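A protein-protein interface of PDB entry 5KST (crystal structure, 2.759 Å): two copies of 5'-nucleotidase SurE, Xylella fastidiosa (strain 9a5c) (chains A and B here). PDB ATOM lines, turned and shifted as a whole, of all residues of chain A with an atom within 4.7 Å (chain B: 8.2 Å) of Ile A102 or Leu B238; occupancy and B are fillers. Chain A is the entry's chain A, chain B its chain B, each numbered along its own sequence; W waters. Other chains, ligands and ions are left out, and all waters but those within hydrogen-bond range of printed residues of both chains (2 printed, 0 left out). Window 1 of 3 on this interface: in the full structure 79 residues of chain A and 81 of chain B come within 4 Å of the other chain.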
ATOM      1  N   ASP A  99     -27.436  19.830  -3.343  1.00  0.00           N
ATOM      2  CA  ASP A  99     -28.037  21.154  -3.284  1.00  0.00           C
ATOM      3  C   ASP A  99     -29.372  21.164  -2.539  1.00  0.00           C
ATOM      4  O   ASP A  99     -29.992  22.220  -2.380  1.00  0.00           O
ATOM      5  CB  ASP A  99     -28.228  21.708  -4.698  1.00  0.00           C
ATOM      6  CG  ASP A  99     -28.409  20.612  -5.745  1.00  0.00           C
ATOM      7  OD1 ASP A  99     -28.744  19.458  -5.385  1.00  0.00           O
ATOM      8  OD2 ASP A  99     -28.218  20.921  -6.939  1.00  0.00           O
ATOM      9  N   ASP A 100     -29.810  19.990  -2.099  1.00  0.00           N
ATOM     10  CA  ASP A 100     -31.041  19.884  -1.336  1.00  0.00           C
ATOM     11  C   ASP A 100     -30.767  20.163   0.129  1.00  0.00           C
ATOM     12  O   ASP A 100     -31.649  20.603   0.858  1.00  0.00           O
ATOM     13  CB  ASP A 100     -31.667  18.499  -1.488  1.00  0.00           C
ATOM     14  CG  ASP A 100     -32.154  18.230  -2.887  1.00  0.00           C
ATOM     15  OD1 ASP A 100     -32.469  19.204  -3.601  1.00  0.00           O
ATOM     16  OD2 ASP A 100     -32.226  17.044  -3.270  1.00  0.00           O
ATOM     17  N   VAL A 101     -29.531  19.900   0.543  1.00  0.00           N
ATOM     18  CA  VAL A 101     -29.117  19.990   1.941  1.00  0.00           C
ATOM     19  C   VAL A 101     -29.492  21.308   2.608  1.00  0.00           C
ATOM     20  O   VAL A 101     -29.965  21.328   3.744  1.00  0.00           O
ATOM     21  CB  VAL A 101     -27.597  19.787   2.066  1.00  0.00           C
ATOM     22  CG1 VAL A 101     -27.127  20.042   3.489  1.00  0.00           C
ATOM     23  CG2 VAL A 101     -27.231  18.388   1.620  1.00  0.00           C
ATOM     24  N   ILE A 102     -29.307  22.403   1.883  1.00  0.00           N
ATOM     25  CA  ILE A 102     -29.486  23.732   2.443  1.00  0.00           C
ATOM     26  C   ILE A 102     -30.926  23.990   2.909  1.00  0.00           C
ATOM     27  O   ILE A 102     -31.151  24.794   3.812  1.00  0.00           O
ATOM     28  CB  ILE A 102     -29.044  24.807   1.420  1.00  0.00           C
ATOM     29  CG1 ILE A 102     -29.028  26.192   2.060  1.00  0.00           C
ATOM     30  CG2 ILE A 102     -29.917  24.777   0.170  1.00  0.00           C
ATOM     31  CD1 ILE A 102     -28.470  27.257   1.157  1.00  0.00           C
ATOM     32  N   TYR A 103     -31.896  23.287   2.331  1.00  0.00           N
ATOM     33  CA  TYR A 103     -33.293  23.512   2.698  1.00  0.00           C
ATOM     34  C   TYR A 103     -33.892  22.364   3.483  1.00  0.00           C
ATOM     35  O   TYR A 103     -35.088  22.358   3.768  1.00  0.00           O
ATOM     36  CB  TYR A 103     -34.116  23.784   1.447  1.00  0.00           C
ATOM     37  CG  TYR A 103     -33.603  25.005   0.746  1.00  0.00           C
ATOM     38  CD1 TYR A 103     -33.268  26.140   1.478  1.00  0.00           C
ATOM     39  CD2 TYR A 103     -33.393  25.016  -0.626  1.00  0.00           C
ATOM     40  CE1 TYR A 103     -32.771  27.265   0.865  1.00  0.00           C
ATOM     41  CE2 TYR A 103     -32.892  26.142  -1.254  1.00  0.00           C
ATOM     42  CZ  TYR A 103     -32.585  27.261  -0.498  1.00  0.00           C
ATOM     43  OH  TYR A 103     -32.082  28.385  -1.096  1.00  0.00           O
ATOM     44  N   SER A 104     -33.048  21.406   3.847  1.00  0.00           N
ATOM     45  CA  SER A 104     -33.479  20.252   4.622  1.00  0.00           C
ATOM     46  C   SER A 104     -33.900  20.627   6.042  1.00  0.00           C
ATOM     47  O   SER A 104     -33.184  21.337   6.746  1.00  0.00           O
ATOM     48  CB  SER A 104     -32.366  19.209   4.674  1.00  0.00           C
ATOM     49  OG  SER A 104     -32.644  18.218   5.653  1.00  0.00           O
ATOM     50  N   MET A 111     -28.157  22.669  12.112  1.00  0.00           N
ATOM     51  CA  MET A 111     -27.701  24.036  11.911  1.00  0.00           C
ATOM     52  C   MET A 111     -27.843  24.843  13.192  1.00  0.00           C
ATOM     53  O   MET A 111     -26.904  25.500  13.638  1.00  0.00           O
ATOM     54  CB  MET A 111     -28.499  24.706  10.791  1.00  0.00           C
ATOM     55  CG  MET A 111     -28.179  24.220   9.402  1.00  0.00           C
ATOM     56  SD  MET A 111     -26.708  25.026   8.799  1.00  0.00           S
ATOM     57  CE  MET A 111     -26.445  24.155   7.260  1.00  0.00           C
ATOM     58  N   LEU A 183     -20.732  18.299  -1.188  1.00  0.00           N
ATOM     59  CA  LEU A 183     -22.095  18.360  -1.695  1.00  0.00           C
ATOM     60  C   LEU A 183     -22.101  18.251  -3.207  1.00  0.00           C
ATOM     61  O   LEU A 183     -21.323  18.911  -3.895  1.00  0.00           O
ATOM     62  CB  LEU A 183     -22.787  19.651  -1.260  1.00  0.00           C
ATOM     63  CG  LEU A 183     -23.075  19.755   0.231  1.00  0.00           C
ATOM     64  CD1 LEU A 183     -23.909  20.990   0.518  1.00  0.00           C
ATOM     65  CD2 LEU A 183     -23.780  18.498   0.708  1.00  0.00           C
ATOM     66  N   PRO A 233     -18.983  17.444   5.787  1.00  0.00           N
ATOM     67  CA  PRO A 233     -18.857  18.588   6.691  1.00  0.00           C
ATOM     68  C   PRO A 233     -19.397  19.820   5.985  1.00  0.00           C
ATOM     69  O   PRO A 233     -18.990  20.094   4.858  1.00  0.00           O
ATOM     70  CB  PRO A 233     -17.350  18.689   6.933  1.00  0.00           C
ATOM     71  CG  PRO A 233     -16.740  18.104   5.696  1.00  0.00           C
ATOM     72  CD  PRO A 233     -17.680  17.008   5.255  1.00  0.00           C
ATOM     73  N   ILE A 234     -20.323  20.540   6.604  1.00  0.00           N
ATOM     74  CA  ILE A 234     -20.879  21.695   5.919  1.00  0.00           C
ATOM     75  C   ILE A 234     -20.839  22.972   6.751  1.00  0.00           C
ATOM     76  O   ILE A 234     -20.907  22.936   7.982  1.00  0.00           O
ATOM     77  CB  ILE A 234     -22.337  21.437   5.468  1.00  0.00           C
ATOM     78  CG1 ILE A 234     -23.245  21.241   6.671  1.00  0.00           C
ATOM     79  CG2 ILE A 234     -22.418  20.222   4.568  1.00  0.00           C
ATOM     80  CD1 ILE A 234     -24.660  20.912   6.296  1.00  0.00           C
ATOM     81  N   HIS A 235     -20.704  24.096   6.050  1.00  0.00           N
ATOM     82  CA  HIS A 235     -20.793  25.428   6.636  1.00  0.00           C
ATOM     83  C   HIS A 235     -22.079  25.625   7.413  1.00  0.00           C
ATOM     84  O   HIS A 235     -23.132  25.130   7.027  1.00  0.00           O
ATOM     85  CB  HIS A 235     -20.730  26.502   5.555  1.00  0.00           C
ATOM     86  CG  HIS A 235     -19.382  26.675   4.937  1.00  0.00           C
ATOM     87  ND1 HIS A 235     -18.314  27.212   5.620  1.00  0.00           N
ATOM     88  CD2 HIS A 235     -18.939  26.418   3.682  1.00  0.00           C
ATOM     89  CE1 HIS A 235     -17.263  27.259   4.819  1.00  0.00           C
ATOM     90  NE2 HIS A 235     -17.616  26.780   3.640  1.00  0.00           N
ATOM     91  N   LEU A 238     -22.703  30.936   6.280  1.00  0.00           N
ATOM     92  CA  LEU A 238     -22.791  31.032   4.828  1.00  0.00           C
ATOM     93  C   LEU A 238     -21.860  32.092   4.255  1.00  0.00           C
ATOM     94  O   LEU A 238     -21.636  32.120   3.053  1.00  0.00           O
ATOM     95  CB  LEU A 238     -24.225  31.326   4.388  1.00  0.00           C
ATOM     96  CG  LEU A 238     -25.282  30.302   4.793  1.00  0.00           C
ATOM     97  CD1 LEU A 238     -26.501  30.431   3.903  1.00  0.00           C
ATOM     98  CD2 LEU A 238     -24.725  28.893   4.748  1.00  0.00           C
ATOM     99  N   ASN B  44     -38.321  26.410   1.170  1.00  0.00           N
ATOM    100  CA  ASN B  44     -37.652  26.998   0.019  1.00  0.00           C
ATOM    101  C   ASN B  44     -37.297  25.985  -1.067  1.00  0.00           C
ATOM    102  O   ASN B  44     -37.146  26.349  -2.233  1.00  0.00           O
ATOM    103  CB  ASN B  44     -36.392  27.730   0.471  1.00  0.00           C
ATOM    104  CG  ASN B  44     -36.703  29.003   1.227  1.00  0.00           C
ATOM    105  OD1 ASN B  44     -37.729  29.646   0.985  1.00  0.00           O
ATOM    106  ND2 ASN B  44     -35.818  29.377   2.146  1.00  0.00           N
ATOM    107  N   SER B  45     -37.174  24.722  -0.680  1.00  0.00           N
ATOM    108  CA  SER B  45     -36.759  23.656  -1.587  1.00  0.00           C
ATOM    109  C   SER B  45     -37.602  23.550  -2.856  1.00  0.00           C
ATOM    110  O   SER B  45     -38.782  23.908  -2.866  1.00  0.00           O
ATOM    111  CB  SER B  45     -36.795  22.325  -0.848  1.00  0.00           C
ATOM    112  OG  SER B  45     -37.980  22.249  -0.082  1.00  0.00           O
ATOM    113  N   THR B  69     -37.393  29.260  -5.306  1.00  0.00           N
ATOM    114  CA  THR B  69     -36.426  28.431  -6.007  1.00  0.00           C
ATOM    115  C   THR B  69     -37.083  27.809  -7.216  1.00  0.00           C
ATOM    116  O   THR B  69     -36.444  27.668  -8.254  1.00  0.00           O
ATOM    117  CB  THR B  69     -35.844  27.320  -5.111  1.00  0.00           C
ATOM    118  OG1 THR B  69     -36.904  26.504  -4.605  1.00  0.00           O
ATOM    119  CG2 THR B  69     -35.067  27.922  -3.950  1.00  0.00           C
ATOM    120  N   VAL B 101     -30.342  34.343   7.236  1.00  0.00           N
ATOM    121  CA  VAL B 101     -30.101  34.316   5.794  1.00  0.00           C
ATOM    122  C   VAL B 101     -30.326  32.941   5.175  1.00  0.00           C
ATOM    123  O   VAL B 101     -30.927  32.820   4.106  1.00  0.00           O
ATOM    124  CB  VAL B 101     -28.666  34.781   5.477  1.00  0.00           C
ATOM    125  CG1 VAL B 101     -28.342  34.606   4.005  1.00  0.00           C
ATOM    126  CG2 VAL B 101     -28.493  36.222   5.887  1.00  0.00           C
ATOM    127  N   ILE B 102     -29.867  31.907   5.868  1.00  0.00           N
ATOM    128  CA  ILE B 102     -29.873  30.559   5.320  1.00  0.00           C
ATOM    129  C   ILE B 102     -31.289  30.039   5.033  1.00  0.00           C
ATOM    130  O   ILE B 102     -31.478  29.183   4.165  1.00  0.00           O
ATOM    131  CB  ILE B 102     -29.127  29.586   6.269  1.00  0.00           C
ATOM    132  CG1 ILE B 102     -28.945  28.219   5.609  1.00  0.00           C
ATOM    133  CG2 ILE B 102     -29.826  29.481   7.612  1.00  0.00           C
ATOM    134  CD1 ILE B 102     -28.081  27.286   6.410  1.00  0.00           C
ATOM    135  N   TYR B 103     -32.288  30.579   5.725  1.00  0.00           N
ATOM    136  CA  TYR B 103     -33.660  30.112   5.543  1.00  0.00           C
ATOM    137  C   TYR B 103     -34.544  31.144   4.860  1.00  0.00           C
ATOM    138  O   TYR B 103     -35.754  30.955   4.729  1.00  0.00           O
ATOM    139  CB  TYR B 103     -34.250  29.708   6.888  1.00  0.00           C
ATOM    140  CG  TYR B 103     -33.443  28.601   7.501  1.00  0.00           C
ATOM    141  CD1 TYR B 103     -33.014  27.533   6.720  1.00  0.00           C
ATOM    142  CD2 TYR B 103     -33.060  28.640   8.837  1.00  0.00           C
ATOM    143  CE1 TYR B 103     -32.253  26.519   7.254  1.00  0.00           C
ATOM    144  CE2 TYR B 103     -32.297  27.626   9.385  1.00  0.00           C
ATOM    145  CZ  TYR B 103     -31.898  26.570   8.584  1.00  0.00           C
ATOM    146  OH  TYR B 103     -31.135  25.559   9.104  1.00  0.00           O
ATOM    147  N   SER B 104     -33.925  32.227   4.409  1.00  0.00           N
ATOM    148  CA  SER B 104     -34.642  33.268   3.692  1.00  0.00           C
ATOM    149  C   SER B 104     -35.162  32.804   2.337  1.00  0.00           C
ATOM    150  O   SER B 104     -34.425  32.222   1.544  1.00  0.00           O
ATOM    151  CB  SER B 104     -33.742  34.489   3.498  1.00  0.00           C
ATOM    152  OG  SER B 104     -34.317  35.408   2.582  1.00  0.00           O
ATOM    153  N   VAL B 107     -33.374  34.884  -0.363  1.00  0.00           N
ATOM    154  CA  VAL B 107     -32.036  34.383  -0.621  1.00  0.00           C
ATOM    155  C   VAL B 107     -32.106  33.078  -1.396  1.00  0.00           C
ATOM    156  O   VAL B 107     -31.249  32.802  -2.232  1.00  0.00           O
ATOM    157  CB  VAL B 107     -31.253  34.185   0.689  1.00  0.00           C
ATOM    158  CG1 VAL B 107     -29.875  33.594   0.416  1.00  0.00           C
ATOM    159  CG2 VAL B 107     -31.131  35.512   1.424  1.00  0.00           C
ATOM    160  N   SER B 108     -33.155  32.299  -1.139  1.00  0.00           N
ATOM    161  CA  SER B 108     -33.311  30.993  -1.768  1.00  0.00           C
ATOM    162  C   SER B 108     -33.373  31.097  -3.284  1.00  0.00           C
ATOM    163  O   SER B 108     -32.801  30.269  -3.993  1.00  0.00           O
ATOM    164  CB  SER B 108     -34.563  30.286  -1.247  1.00  0.00           C
ATOM    165  OG  SER B 108     -35.724  30.731  -1.925  1.00  0.00           O
ATOM    166  N   MET B 111     -29.987  31.729  -4.441  1.00  0.00           N
ATOM    167  CA  MET B 111     -29.286  30.457  -4.311  1.00  0.00           C
ATOM    168  C   MET B 111     -29.443  29.621  -5.557  1.00  0.00           C
ATOM    169  O   MET B 111     -28.469  29.120  -6.115  1.00  0.00           O
ATOM    170  CB  MET B 111     -29.815  29.670  -3.113  1.00  0.00           C
ATOM    171  CG  MET B 111     -29.389  30.195  -1.768  1.00  0.00           C
ATOM    172  SD  MET B 111     -27.721  29.661  -1.373  1.00  0.00           S
ATOM    173  CE  MET B 111     -27.423  30.607   0.119  1.00  0.00           C
ATOM    174  N   GLU B 112     -30.689  29.472  -5.989  1.00  0.00           N
ATOM    175  CA  GLU B 112     -30.996  28.626  -7.125  1.00  0.00           C
ATOM    176  C   GLU B 112     -30.355  29.188  -8.384  1.00  0.00           C
ATOM    177  O   GLU B 112     -29.875  28.439  -9.229  1.00  0.00           O
ATOM    178  CB  GLU B 112     -32.506  28.488  -7.293  1.00  0.00           C
ATOM    179  CG  GLU B 112     -32.929  27.429  -8.295  1.00  0.00           C
ATOM    180  CD  GLU B 112     -32.536  26.011  -7.889  1.00  0.00           C
ATOM    181  OE1 GLU B 112     -32.019  25.819  -6.766  1.00  0.00           O
ATOM    182  OE2 GLU B 112     -32.749  25.080  -8.704  1.00  0.00           O
ATOM    183  N   PHE B 115     -26.884  28.029  -8.179  1.00  0.00           N
ATOM    184  CA  PHE B 115     -26.914  26.592  -8.409  1.00  0.00           C
ATOM    185  C   PHE B 115     -26.998  26.283  -9.898  1.00  0.00           C
ATOM    186  O   PHE B 115     -26.370  25.339 -10.376  1.00  0.00           O
ATOM    187  CB  PHE B 115     -28.093  25.950  -7.679  1.00  0.00           C
ATOM    188  CG  PHE B 115     -27.838  25.680  -6.226  1.00  0.00           C
ATOM    189  CD1 PHE B 115     -26.549  25.494  -5.758  1.00  0.00           C
ATOM    190  CD2 PHE B 115     -28.891  25.604  -5.329  1.00  0.00           C
ATOM    191  CE1 PHE B 115     -26.314  25.243  -4.419  1.00  0.00           C
ATOM    192  CE2 PHE B 115     -28.664  25.348  -3.990  1.00  0.00           C
ATOM    193  CZ  PHE B 115     -27.373  25.165  -3.535  1.00  0.00           C
ATOM    194  N   ASP B 160     -19.380  29.857  -6.912  1.00  0.00           N
ATOM    195  CA  ASP B 160     -20.409  29.486  -5.947  1.00  0.00           C
ATOM    196  C   ASP B 160     -20.624  30.578  -4.905  1.00  0.00           C
ATOM    197  O   ASP B 160     -20.624  30.312  -3.701  1.00  0.00           O
ATOM    198  CB  ASP B 160     -20.050  28.157  -5.270  1.00  0.00           C
ATOM    199  N   ILE B 162     -23.120  34.125  -4.052  1.00  0.00           N
ATOM    200  CA  ILE B 162     -24.114  35.155  -4.287  1.00  0.00           C
ATOM    201  C   ILE B 162     -23.954  36.267  -3.254  1.00  0.00           C
ATOM    202  O   ILE B 162     -23.350  36.069  -2.196  1.00  0.00           O
ATOM    203  CB  ILE B 162     -25.556  34.605  -4.234  1.00  0.00           C
ATOM    204  CG1 ILE B 162     -25.942  34.228  -2.809  1.00  0.00           C
ATOM    205  CG2 ILE B 162     -25.705  33.424  -5.136  1.00  0.00           C
ATOM    206  CD1 ILE B 162     -27.289  33.555  -2.698  1.00  0.00           C
ATOM    207  N   ILE B 234     -22.003  35.254   0.029  1.00  0.00           N
ATOM    208  CA  ILE B 234     -22.264  34.036   0.772  1.00  0.00           C
ATOM    209  C   ILE B 234     -22.116  32.770  -0.061  1.00  0.00           C
ATOM    210  O   ILE B 234     -22.348  32.776  -1.265  1.00  0.00           O
ATOM    211  CB  ILE B 234     -23.676  34.049   1.405  1.00  0.00           C
ATOM    212  CG1 ILE B 234     -24.747  34.069   0.334  1.00  0.00           C
ATOM    213  CG2 ILE B 234     -23.854  35.246   2.324  1.00  0.00           C
ATOM    214  CD1 ILE B 234     -26.131  34.133   0.899  1.00  0.00           C
ATOM    215  N   HIS B 235     -21.704  31.694   0.605  1.00  0.00           N
ATOM    216  CA  HIS B 235     -21.620  30.366   0.009  1.00  0.00           C
ATOM    217  C   HIS B 235     -22.939  29.938  -0.610  1.00  0.00           C
ATOM    218  O   HIS B 235     -24.004  30.235  -0.075  1.00  0.00           O
ATOM    219  CB  HIS B 235     -21.230  29.326   1.062  1.00  0.00           C
ATOM    220  CG  HIS B 235     -19.803  29.398   1.506  1.00  0.00           C
ATOM    221  ND1 HIS B 235     -18.751  29.067   0.682  1.00  0.00           N
ATOM    222  CD2 HIS B 235     -19.258  29.729   2.700  1.00  0.00           C
ATOM    223  CE1 HIS B 235     -17.615  29.209   1.344  1.00  0.00           C
ATOM    224  NE2 HIS B 235     -17.895  29.609   2.570  1.00  0.00           N
ATOM    225  N   VAL B 236     -22.882  29.228  -1.729  1.00  0.00           N
ATOM    226  CA  VAL B 236     -24.044  28.454  -2.142  1.00  0.00           C
ATOM    227  C   VAL B 236     -23.672  26.989  -1.991  1.00  0.00           C
ATOM    228  O   VAL B 236     -24.536  26.125  -1.859  1.00  0.00           O
ATOM    229  CB  VAL B 236     -24.501  28.758  -3.576  1.00  0.00           C
ATOM    230  CG1 VAL B 236     -24.635  30.250  -3.756  1.00  0.00           C
ATOM    231  CG2 VAL B 236     -23.549  28.157  -4.596  1.00  0.00           C
ATOM    232  N   ASP B 237     -22.368  26.728  -1.986  1.00  0.00           N
ATOM    233  CA  ASP B 237     -21.859  25.409  -1.664  1.00  0.00           C
ATOM    234  C   ASP B 237     -21.589  25.324  -0.161  1.00  0.00           C
ATOM    235  O   ASP B 237     -20.606  25.878   0.338  1.00  0.00           O
ATOM    236  CB  ASP B 237     -20.592  25.105  -2.460  1.00  0.00           C
ATOM    237  CG  ASP B 237     -20.168  23.654  -2.346  1.00  0.00           C
ATOM    238  OD1 ASP B 237     -20.728  22.935  -1.491  1.00  0.00           O
ATOM    239  OD2 ASP B 237     -19.274  23.231  -3.107  1.00  0.00           O
ATOM    240  N   LEU B 238     -22.461  24.620   0.551  1.00  0.00           N
ATOM    241  CA  LEU B 238     -22.347  24.532   2.000  1.00  0.00           C
ATOM    242  C   LEU B 238     -21.175  23.661   2.438  1.00  0.00           C
ATOM    243  O   LEU B 238     -20.809  23.672   3.605  1.00  0.00           O
ATOM    244  CB  LEU B 238     -23.640  23.996   2.611  1.00  0.00           C
ATOM    245  CG  LEU B 238     -24.908  24.810   2.351  1.00  0.00           C
ATOM    246  CD1 LEU B 238     -25.978  24.486   3.381  1.00  0.00           C
ATOM    247  CD2 LEU B 238     -24.600  26.286   2.357  1.00  0.00           C
ATOM    248  N   THR B 239     -20.587  22.916   1.505  1.00  0.00           N
ATOM    249  CA  THR B 239     -19.482  22.023   1.829  1.00  0.00           C
ATOM    250  C   THR B 239     -18.345  22.747   2.522  1.00  0.00           C
ATOM    251  O   THR B 239     -17.715  23.623   1.945  1.00  0.00           O
ATOM    252  CB  THR B 239     -18.911  21.335   0.579  1.00  0.00           C
ATOM    253  OG1 THR B 239     -19.920  20.513  -0.022  1.00  0.00           O
ATOM    254  CG2 THR B 239     -17.708  20.471   0.951  1.00  0.00           C
ATOM    255  N   ARG B 240     -18.088  22.375   3.768  1.00  0.00           N
ATOM    256  CA  ARG B 240     -16.953  22.904   4.503  1.00  0.00           C
ATOM    257  C   ARG B 240     -15.677  22.233   4.012  1.00  0.00           C
ATOM    258  O   ARG B 240     -15.204  21.270   4.615  1.00  0.00           O
ATOM    259  CB  ARG B 240     -17.136  22.684   6.004  1.00  0.00           C
ATOM    260  CG  ARG B 240     -16.149  23.428   6.882  1.00  0.00           C
ATOM    261  CD  ARG B 240     -16.618  24.832   7.185  1.00  0.00           C
ATOM    262  NE  ARG B 240     -15.825  25.441   8.249  1.00  0.00           N
ATOM    263  CZ  ARG B 240     -14.708  26.133   8.052  1.00  0.00           C
ATOM    264  NH1 ARG B 240     -14.244  26.317   6.824  1.00  0.00           N
ATOM    265  NH2 ARG B 240     -14.058  26.644   9.088  1.00  0.00           N
ATOM    266  N   TYR B 241     -15.128  22.738   2.912  1.00  0.00           N
ATOM    267  CA  TYR B 241     -13.968  22.117   2.282  1.00  0.00           C
ATOM    268  C   TYR B 241     -12.745  22.061   3.197  1.00  0.00           C
ATOM    269  O   TYR B 241     -12.020  21.068   3.198  1.00  0.00           O
ATOM    270  CB  TYR B 241     -13.615  22.845   0.982  1.00  0.00           C
ATOM    271  CG  TYR B 241     -14.604  22.591  -0.134  1.00  0.00           C
ATOM    272  CD1 TYR B 241     -14.543  21.424  -0.890  1.00  0.00           C
ATOM    273  CD2 TYR B 241     -15.607  23.510  -0.429  1.00  0.00           C
ATOM    274  CE1 TYR B 241     -15.448  21.178  -1.906  1.00  0.00           C
ATOM    275  CE2 TYR B 241     -16.521  23.272  -1.449  1.00  0.00           C
ATOM    276  CZ  TYR B 241     -16.432  22.101  -2.184  1.00  0.00           C
ATOM    277  OH  TYR B 241     -17.328  21.850  -3.198  1.00  0.00           O
HETATM  278  O   HOH W   1     -31.458  23.517   6.653  1.00  0.00           O
HETATM  279  O   HOH W   2     -26.939  22.302  -8.856  1.00  0.00           O
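The side-chain hydroxyl (OG1) of Thr B239 lies within hydrogen-bond range of the backbone NH (N) of Leu A183, 2.6 Å away. O of Pro A233 sits at hydrogen-bond distance from N of Arg B240, at 2.7 Å. NE2 of His B235 is in hydrogen-bond range of NE2 of His A235. The backbone NH (N) of His A235 sits at hydrogen-bond distance from the backbone carbonyl oxygen (O) of Leu B238, at 2.5 Å. The backbone carbonyl oxygen (O) of Leu A238 lies within hydrogen-bond range of the backbone NH (N) of His B235, at 2.5 Å.
The side-chain amide nitrogen (ND2) of Asn B44 lies within hydrogen-bond range of the backbone carbonyl oxygen (O) of Tyr B103, at 3.0 Å. The side-chain amide nitrogen of Asn B44 sits at hydrogen-bond distance from the backbone carbonyl oxygen of Ser B104, at 3.2 Å. O of Ile B162 is in hydrogen-bond range of N of Ile B234, at 2.7 Å. The side-chain carboxylate (OD1) of Asp B237 is in hydrogen-bond range of the side-chain hydroxyl (OG1) of Thr B239 (2.9 Å).
CB of Asp A99 touches CE2 of Phe B115, 3.7 Å away. Ile A102 touches Met B111 (CD1 to SD, 3.6 Å). Tyr A103 touches Ser B108. Met B111 touches Tyr A103 (CB to OH, 3.3 Å). Tyr B103 touches Met A111. CD1 of Leu A183 touches CB of Leu B238, 3.7 Å away. C of Thr B239 touches O of Pro A233 (3.6 Å). His A235 touches Arg B240. Leu A238 touches Ile B102. Leu A238 touches Ile B234 (O to CA, 3.0 Å).
Printed residues of chain B within 4 Å of Ile A102: Met B111 (3.6 Å) and Leu B238 (3.7 Å). Leu B238 touches six residues of chain A. Printed residues of chain A within 4 Å of His B235: His A235 and Leu A238. Of the printed residues of chain A, Ser B45 touches Tyr A103 (3.8 Å). Of the printed residues of chain B, Met A111 touches Ile B102 (3.6 Å), Tyr B103 (3.2 Å) and Leu B238 (3.9 Å). Of the printed residues of chain A, Phe B115 touches Asp A99. Of the printed residues of chain B, Ile A234 touches Leu B238 and Arg B240. Ile B162 touches none of the printed residues of chain A. The nearest printed residue of chain B that does not touch Ile A102 is Tyr B103 (4.005 Å). The nearest residue of chain A that does not touch Leu B238 is Pro A233 (4.2 Å). The nearest printed residue of chain B that does not touch Met A111 is Thr B239 (8.3 Å).
Hydrophobic or aromatic side chains of chain A that line the printed part of chain B: Ile A102, Tyr A103, Met A111, Leu A183, Pro A233, Ile A234, His A235 and Leu A238. Of the 22 printed residues of chain B, 14 touch a printed residue of chain A. Hydrophobic or aromatic side chains of chain B within 4 Å of the printed part of chain A: Ile B102, Tyr B103, Met B111, Phe B115, Ile B234, His B235 and Leu B238.
Ile A102 touches Leu B238, and with the chains exchanged Leu A238 touches Ile B102. Met A111 touches Leu B238, and with the chains exchanged Leu A238 touches Met B111. Ile A234 touches Leu B238, and with the chains exchanged Leu A238 touches Ile B234. His B235 touches its own counterpart, His A235. Positions printed for both chains: 101, 102, 103, 104, 111, 234, 235 and 238. Of the 28 pairs that touch across the chains among the printed residues, 14 have their exchanged pair printed and touching as well.
Water W2 lies within hydrogen-bond range of OD2 of Asp A99 and O of Phe B115. Water W1 lies within hydrogen-bond range of O of Ser A104, O of Ile A102 and OH of Tyr B103.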
